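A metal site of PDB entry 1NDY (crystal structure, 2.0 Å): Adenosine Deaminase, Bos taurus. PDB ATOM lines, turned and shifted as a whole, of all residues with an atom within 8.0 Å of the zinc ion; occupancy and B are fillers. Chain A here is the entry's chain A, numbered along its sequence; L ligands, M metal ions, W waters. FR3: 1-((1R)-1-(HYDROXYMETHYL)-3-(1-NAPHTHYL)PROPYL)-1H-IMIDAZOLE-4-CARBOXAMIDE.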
ATOM      1  N   HIS A  14     -20.562  -5.838   7.875  1.00  0.00           N
ATOM      2  CA  HIS A  14     -21.470  -6.683   8.655  1.00  0.00           C
ATOM      3  C   HIS A  14     -20.606  -7.340   9.833  1.00  0.00           C
ATOM      4  O   HIS A  14     -20.037  -8.424   9.597  1.00  0.00           O
ATOM      5  CB  HIS A  14     -22.151  -7.810   7.785  1.00  0.00           C
ATOM      6  CG  HIS A  14     -23.402  -8.390   8.545  1.00  0.00           C
ATOM      7  ND1 HIS A  14     -24.622  -8.359   8.125  1.00  0.00           N
ATOM      8  CD2 HIS A  14     -23.431  -9.130   9.759  1.00  0.00           C
ATOM      9  CE1 HIS A  14     -25.477  -9.003   8.975  1.00  0.00           C
ATOM     10  NE2 HIS A  14     -24.745  -9.512  10.019  1.00  0.00           N
ATOM     11  N   VAL A  15     -20.580  -6.661  10.987  1.00  0.00           N
ATOM     12  CA  VAL A  15     -19.872  -7.257  12.126  1.00  0.00           C
ATOM     13  C   VAL A  15     -20.604  -6.546  13.328  1.00  0.00           C
ATOM     14  O   VAL A  15     -20.932  -5.353  13.331  1.00  0.00           O
ATOM     15  CB  VAL A  15     -18.335  -6.904  12.088  1.00  0.00           C
ATOM     16  CG1 VAL A  15     -18.014  -5.406  11.764  1.00  0.00           C
ATOM     17  CG2 VAL A  15     -17.702  -7.393  13.423  1.00  0.00           C
ATOM     18  N   HIS A  16     -21.021  -7.462  14.232  1.00  0.00           N
ATOM     19  CA  HIS A  16     -21.676  -6.923  15.411  1.00  0.00           C
ATOM     20  C   HIS A  16     -20.600  -6.673  16.561  1.00  0.00           C
ATOM     21  O   HIS A  16     -19.838  -7.576  17.038  1.00  0.00           O
ATOM     22  CB  HIS A  16     -22.571  -8.129  15.984  1.00  0.00           C
ATOM     23  CG  HIS A  16     -23.694  -8.604  15.043  1.00  0.00           C
ATOM     24  ND1 HIS A  16     -24.937  -8.290  15.261  1.00  0.00           N
ATOM     25  CD2 HIS A  16     -23.655  -9.349  13.849  1.00  0.00           C
ATOM     26  CE1 HIS A  16     -25.748  -8.830  14.261  1.00  0.00           C
ATOM     27  NE2 HIS A  16     -24.978  -9.484  13.362  1.00  0.00           N
ATOM     28  N   ARG A 100     -22.245  -2.734  13.972  1.00  0.00           N
ATOM     29  CA  ARG A 100     -23.639  -2.694  14.454  1.00  0.00           C
ATOM     30  C   ARG A 100     -23.868  -3.362  15.840  1.00  0.00           C
ATOM     31  O   ARG A 100     -23.007  -4.221  16.209  1.00  0.00           O
ATOM     32  CB  ARG A 100     -24.552  -3.468  13.463  1.00  0.00           C
ATOM     33  CG  ARG A 100     -24.396  -5.024  13.525  1.00  0.00           C
ATOM     34  CD  ARG A 100     -25.077  -5.785  12.312  1.00  0.00           C
ATOM     35  NE  ARG A 100     -24.697  -5.145  11.003  1.00  0.00           N
ATOM     36  CZ  ARG A 100     -25.330  -5.344   9.790  1.00  0.00           C
ATOM     37  NH1 ARG A 100     -26.498  -6.009   9.887  1.00  0.00           N
ATOM     38  NH2 ARG A 100     -24.872  -4.971   8.500  1.00  0.00           N
ATOM     39  N   CYS A 152     -29.392  -1.704  15.792  1.00  0.00           N
ATOM     40  CA  CYS A 152     -30.189  -2.868  15.439  1.00  0.00           C
ATOM     41  C   CYS A 152     -31.462  -2.786  16.276  1.00  0.00           C
ATOM     42  O   CYS A 152     -31.440  -2.736  17.496  1.00  0.00           O
ATOM     43  CB  CYS A 152     -29.465  -4.168  15.831  1.00  0.00           C
ATOM     44  SG  CYS A 152     -27.897  -4.485  14.981  1.00  0.00           S
ATOM     45  N   ASP A 180     -30.671  -1.440  11.483  1.00  0.00           N
ATOM     46  CA  ASP A 180     -30.741  -2.900  11.078  1.00  0.00           C
ATOM     47  C   ASP A 180     -31.880  -3.659  11.949  1.00  0.00           C
ATOM     48  O   ASP A 180     -32.547  -3.070  12.782  1.00  0.00           O
ATOM     49  CB  ASP A 180     -29.356  -3.575  11.286  1.00  0.00           C
ATOM     50  CG  ASP A 180     -29.204  -5.103  11.025  1.00  0.00           C
ATOM     51  OD1 ASP A 180     -28.462  -5.736  11.817  1.00  0.00           O
ATOM     52  OD2 ASP A 180     -29.776  -5.632  10.034  1.00  0.00           O
ATOM     53  N   LEU A 181     -32.220  -4.799  11.394  1.00  0.00           N
ATOM     54  CA  LEU A 181     -33.182  -5.692  12.096  1.00  0.00           C
ATOM     55  C   LEU A 181     -32.371  -7.068  12.270  1.00  0.00           C
ATOM     56  O   LEU A 181     -31.998  -7.781  11.321  1.00  0.00           O
ATOM     57  CB  LEU A 181     -34.466  -5.755  11.265  1.00  0.00           C
ATOM     58  CG  LEU A 181     -35.466  -6.887  11.868  1.00  0.00           C
ATOM     59  CD1 LEU A 181     -35.930  -6.349  13.328  1.00  0.00           C
ATOM     60  CD2 LEU A 181     -36.678  -6.851  10.882  1.00  0.00           C
ATOM     61  N   ALA A 182     -32.068  -7.337  13.532  1.00  0.00           N
ATOM     62  CA  ALA A 182     -31.340  -8.579  13.917  1.00  0.00           C
ATOM     63  C   ALA A 182     -32.185  -9.416  14.944  1.00  0.00           C
ATOM     64  O   ALA A 182     -33.234  -8.987  15.441  1.00  0.00           O
ATOM     65  CB  ALA A 182     -30.091  -8.162  14.711  1.00  0.00           C
ATOM     66  N   GLY A 183     -31.654 -10.590  15.279  1.00  0.00           N
ATOM     67  CA  GLY A 183     -32.241 -11.568  16.292  1.00  0.00           C
ATOM     68  C   GLY A 183     -32.674 -12.772  15.514  1.00  0.00           C
ATOM     69  O   GLY A 183     -32.095 -13.202  14.501  1.00  0.00           O
ATOM     70  N   HIS A 213     -31.160  -8.344   8.466  1.00  0.00           N
ATOM     71  CA  HIS A 213     -30.768  -9.742   8.322  1.00  0.00           C
ATOM     72  C   HIS A 213     -31.861 -10.581   7.760  1.00  0.00           C
ATOM     73  O   HIS A 213     -32.915 -10.529   8.339  1.00  0.00           O
ATOM     74  CB  HIS A 213     -30.501 -10.301   9.827  1.00  0.00           C
ATOM     75  CG  HIS A 213     -29.191  -9.827  10.386  1.00  0.00           C
ATOM     76  ND1 HIS A 213     -28.971  -8.611  10.877  1.00  0.00           N
ATOM     77  CD2 HIS A 213     -28.060 -10.649  10.642  1.00  0.00           C
ATOM     78  CE1 HIS A 213     -27.796  -8.637  11.485  1.00  0.00           C
ATOM     79  NE2 HIS A 213     -27.186  -9.842  11.390  1.00  0.00           N
ATOM     80  N   GLU A 216     -30.758 -15.789   6.084  1.00  0.00           N
ATOM     81  CA  GLU A 216     -29.625 -16.470   6.723  1.00  0.00           C
ATOM     82  C   GLU A 216     -30.025 -17.958   6.989  1.00  0.00           C
ATOM     83  O   GLU A 216     -29.435 -18.885   6.523  1.00  0.00           O
ATOM     84  CB  GLU A 216     -29.024 -15.754   7.982  1.00  0.00           C
ATOM     85  CG  GLU A 216     -27.859 -16.600   8.600  1.00  0.00           C
ATOM     86  CD  GLU A 216     -27.431 -15.917   9.926  1.00  0.00           C
ATOM     87  OE1 GLU A 216     -28.131 -15.040  10.430  1.00  0.00           O
ATOM     88  OE2 GLU A 216     -26.380 -16.219  10.458  1.00  0.00           O
ATOM     89  N   GLY A 236     -28.437  -8.584   5.020  1.00  0.00           N
ATOM     90  CA  GLY A 236     -27.562  -9.378   5.915  1.00  0.00           C
ATOM     91  C   GLY A 236     -27.678 -10.890   5.551  1.00  0.00           C
ATOM     92  O   GLY A 236     -28.675 -11.498   5.827  1.00  0.00           O
ATOM     93  N   HIS A 237     -26.617 -11.419   4.922  1.00  0.00           N
ATOM     94  CA  HIS A 237     -26.494 -12.775   4.381  1.00  0.00           C
ATOM     95  C   HIS A 237     -27.318 -12.918   3.105  1.00  0.00           C
ATOM     96  O   HIS A 237     -26.752 -13.046   2.043  1.00  0.00           O
ATOM     97  CB  HIS A 237     -27.029 -13.917   5.379  1.00  0.00           C
ATOM     98  CG  HIS A 237     -26.256 -13.795   6.625  1.00  0.00           C
ATOM     99  ND1 HIS A 237     -25.000 -14.298   6.820  1.00  0.00           N
ATOM    100  CD2 HIS A 237     -26.691 -13.167   7.792  1.00  0.00           C
ATOM    101  CE1 HIS A 237     -24.616 -14.017   8.119  1.00  0.00           C
ATOM    102  NE2 HIS A 237     -25.653 -13.346   8.731  1.00  0.00           N
ATOM    103  N   GLU A 259     -24.536  -8.931   2.072  1.00  0.00           N
ATOM    104  CA  GLU A 259     -23.497  -8.906   3.110  1.00  0.00           C
ATOM    105  C   GLU A 259     -23.134 -10.322   3.575  1.00  0.00           C
ATOM    106  O   GLU A 259     -23.873 -10.853   4.432  1.00  0.00           O
ATOM    107  CB  GLU A 259     -24.080  -8.136   4.382  1.00  0.00           C
ATOM    108  CG  GLU A 259     -24.548  -6.680   4.076  1.00  0.00           C
ATOM    109  CD  GLU A 259     -25.195  -5.960   5.236  1.00  0.00           C
ATOM    110  OE1 GLU A 259     -25.387  -6.634   6.248  1.00  0.00           O
ATOM    111  OE2 GLU A 259     -25.503  -4.722   5.110  1.00  0.00           O
ATOM    112  N   CYS A 261     -21.182 -13.779   5.079  1.00  0.00           N
ATOM    113  CA  CYS A 261     -20.343 -14.052   6.241  1.00  0.00           C
ATOM    114  C   CYS A 261     -19.998 -15.573   6.072  1.00  0.00           C
ATOM    115  O   CYS A 261     -20.707 -16.434   6.545  1.00  0.00           O
ATOM    116  CB  CYS A 261     -21.067 -13.777   7.582  1.00  0.00           C
ATOM    117  SG  CYS A 261     -21.759 -12.038   7.629  1.00  0.00           S
ATOM    118  N   SER A 264     -18.926 -17.631   9.552  1.00  0.00           N
ATOM    119  CA  SER A 264     -20.203 -17.626  10.300  1.00  0.00           C
ATOM    120  C   SER A 264     -21.250 -18.631   9.780  1.00  0.00           C
ATOM    121  O   SER A 264     -21.811 -19.401  10.562  1.00  0.00           O
ATOM    122  CB  SER A 264     -20.926 -16.287  10.169  1.00  0.00           C
ATOM    123  OG  SER A 264     -22.131 -16.230  10.861  1.00  0.00           O
ATOM    124  N   ASN A 292     -17.560 -10.669   5.211  1.00  0.00           N
ATOM    125  CA  ASN A 292     -17.658 -10.134   6.538  1.00  0.00           C
ATOM    126  C   ASN A 292     -17.473 -11.165   7.682  1.00  0.00           C
ATOM    127  O   ASN A 292     -17.652 -12.366   7.506  1.00  0.00           O
ATOM    128  CB  ASN A 292     -19.083  -9.475   6.722  1.00  0.00           C
ATOM    129  CG  ASN A 292     -19.410  -8.470   5.610  1.00  0.00           C
ATOM    130  OD1 ASN A 292     -19.080  -7.299   5.752  1.00  0.00           O
ATOM    131  ND2 ASN A 292     -19.853  -8.995   4.391  1.00  0.00           N
ATOM    132  N   THR A 293     -17.089 -10.718   8.819  1.00  0.00           N
ATOM    133  CA  THR A 293     -16.881 -11.668   9.984  1.00  0.00           C
ATOM    134  C   THR A 293     -18.054 -12.085  10.788  1.00  0.00           C
ATOM    135  O   THR A 293     -18.072 -13.188  11.301  1.00  0.00           O
ATOM    136  CB  THR A 293     -15.956 -10.976  10.942  1.00  0.00           C
ATOM    137  OG1 THR A 293     -16.249  -9.822  11.814  1.00  0.00           O
ATOM    138  CG2 THR A 293     -14.496 -11.066  10.547  1.00  0.00           C
ATOM    139  N   ASP A 294     -19.094 -11.194  10.793  1.00  0.00           N
ATOM    140  CA  ASP A 294     -20.246 -11.291  11.744  1.00  0.00           C
ATOM    141  C   ASP A 294     -19.952 -11.176  13.223  1.00  0.00           C
ATOM    142  O   ASP A 294     -20.298 -10.208  13.871  1.00  0.00           O
ATOM    143  CB  ASP A 294     -21.051 -12.622  11.439  1.00  0.00           C
ATOM    144  CG  ASP A 294     -22.556 -12.552  11.605  1.00  0.00           C
ATOM    145  OD1 ASP A 294     -23.273 -13.662  11.523  1.00  0.00           O
ATOM    146  OD2 ASP A 294     -23.039 -11.442  11.926  1.00  0.00           O
ATOM    147  N   ASP A 295     -19.336 -12.223  13.808  1.00  0.00           N
ATOM    148  CA  ASP A 295     -19.056 -12.176  15.299  1.00  0.00           C
ATOM    149  C   ASP A 295     -17.661 -12.935  15.487  1.00  0.00           C
ATOM    150  O   ASP A 295     -17.560 -14.099  15.880  1.00  0.00           O
ATOM    151  CB  ASP A 295     -20.067 -13.090  16.110  1.00  0.00           C
ATOM    152  CG  ASP A 295     -21.450 -12.502  15.939  1.00  0.00           C
ATOM    153  OD1 ASP A 295     -21.847 -11.772  16.890  1.00  0.00           O
ATOM    154  OD2 ASP A 295     -22.120 -12.779  14.892  1.00  0.00           O
ATOM    155  N   PHE A 299     -16.982 -16.746  16.778  1.00  0.00           N
ATOM    156  CA  PHE A 299     -16.533 -17.693  15.733  1.00  0.00           C
ATOM    157  C   PHE A 299     -15.056 -18.068  15.685  1.00  0.00           C
ATOM    158  O   PHE A 299     -14.514 -18.704  14.798  1.00  0.00           O
ATOM    159  CB  PHE A 299     -17.066 -17.288  14.249  1.00  0.00           C
ATOM    160  CG  PHE A 299     -18.563 -17.112  14.184  1.00  0.00           C
ATOM    161  CD1 PHE A 299     -19.436 -18.147  14.699  1.00  0.00           C
ATOM    162  CD2 PHE A 299     -19.115 -15.922  13.697  1.00  0.00           C
ATOM    163  CE1 PHE A 299     -20.815 -17.966  14.808  1.00  0.00           C
ATOM    164  CE2 PHE A 299     -20.501 -15.773  13.705  1.00  0.00           C
ATOM    165  CZ  PHE A 299     -21.346 -16.763  14.276  1.00  0.00           C
HETATM  166  C1  FR3 L   1     -26.855 -10.827  16.943  1.00  0.00           C
HETATM  167  N2  FR3 L   1     -26.199  -9.987  17.876  1.00  0.00           N
HETATM  168  C3  FR3 L   1     -24.915 -10.366  17.803  1.00  0.00           C
HETATM  169  N4  FR3 L   1     -24.706 -11.390  16.934  1.00  0.00           N
HETATM  170  C5  FR3 L   1     -25.967 -11.649  16.416  1.00  0.00           C
HETATM  171  C8  FR3 L   1     -26.107 -12.691  15.381  1.00  0.00           C
HETATM  172  O9  FR3 L   1     -27.218 -13.102  15.149  1.00  0.00           O
HETATM  173  N10 FR3 L   1     -25.058 -13.325  14.813  1.00  0.00           N
HETATM  174  C13 FR3 L   1     -26.800  -9.112  18.976  1.00  0.00           C
HETATM  175  C14 FR3 L   1     -26.959  -7.551  18.456  1.00  0.00           C
HETATM  176  O15 FR3 L   1     -25.751  -7.108  17.700  1.00  0.00           O
HETATM  177  C18 FR3 L   1     -28.208  -9.565  19.342  1.00  0.00           C
HETATM  178  C19 FR3 L   1     -28.062 -10.939  20.126  1.00  0.00           C
HETATM  179  C22 FR3 L   1     -29.435 -11.534  20.453  1.00  0.00           C
HETATM  180  C25 FR3 L   1     -30.188 -11.050  21.525  1.00  0.00           C
HETATM  181  C26 FR3 L   1     -31.484 -11.566  21.799  1.00  0.00           C
HETATM  182  C27 FR3 L   1     -32.038 -12.534  20.912  1.00  0.00           C
HETATM  183  C28 FR3 L   1     -31.276 -13.017  19.843  1.00  0.00           C
HETATM  184  C29 FR3 L   1     -30.018 -12.471  19.539  1.00  0.00           C
HETATM  185  C2  FR3 L   1     -31.871 -13.941  18.927  1.00  0.00           C
HETATM  186  C4  FR3 L   1     -29.253 -12.959  18.462  1.00  0.00           C
HETATM  187  C6  FR3 L   1     -31.117 -14.422  17.811  1.00  0.00           C
HETATM  188  C7  FR3 L   1     -29.808 -13.878  17.587  1.00  0.00           C
HETATM  189 ZN    ZN M   1     -25.090 -10.551  11.713  1.00  0.00          ZN
HETATM  190  O   HOH W   1     -25.524 -12.487  11.405  1.00  0.00           O
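ND1 of His 16 is in hydrogen-bond range of O15 of the ligand, 2.8 Å away. A nitrogen (N4) of the ligand sits at hydrogen-bond distance from the side-chain carboxylate (OD1) of Asp 295 (2.9 Å).
Within 4 Å of the zinc ion: His 14, His 16, His 213 and Asp 294. The nearest printed residue that does not touch the zinc ion is His 237 (4.1 Å).
The zinc ion is bound by a ring nitrogen (NE2) of His 16 (2.0 Å), water W1 (2.0 Å), a ring nitrogen (NE2) of His 14 (2.0 Å), a ring nitrogen (NE2) of His 213 (2.2 Å) and the side-chain carboxylate of Asp 294 (2.2 Å).
NH2 of Arg 100 is in hydrogen-bond range of ND1 of His 14 (3.4 Å). OE1 of Glu 259 sits at hydrogen-bond distance from ND1 of His 14 (2.7 Å). The side-chain amide oxygen (OD1) of Asn 292 is in hydrogen-bond range of the backbone NH (N) of His 14 (3.0 Å). OD1 of Asp 180 sits close to ND1 of His 213 (3.1 Å). The backbone carbonyl oxygen (O) of Leu 181 sits at hydrogen-bond distance from the backbone NH (N) of His 213. The side-chain hydroxyl (OG) of Ser 264 is in hydrogen-bond range of the side-chain carboxylate (OD1) of Asp 294 (2.9 Å).
Water W1 bridges OD1 of Asp 294 (2.5 Å) and NE2 of His 237 (2.8 Å).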
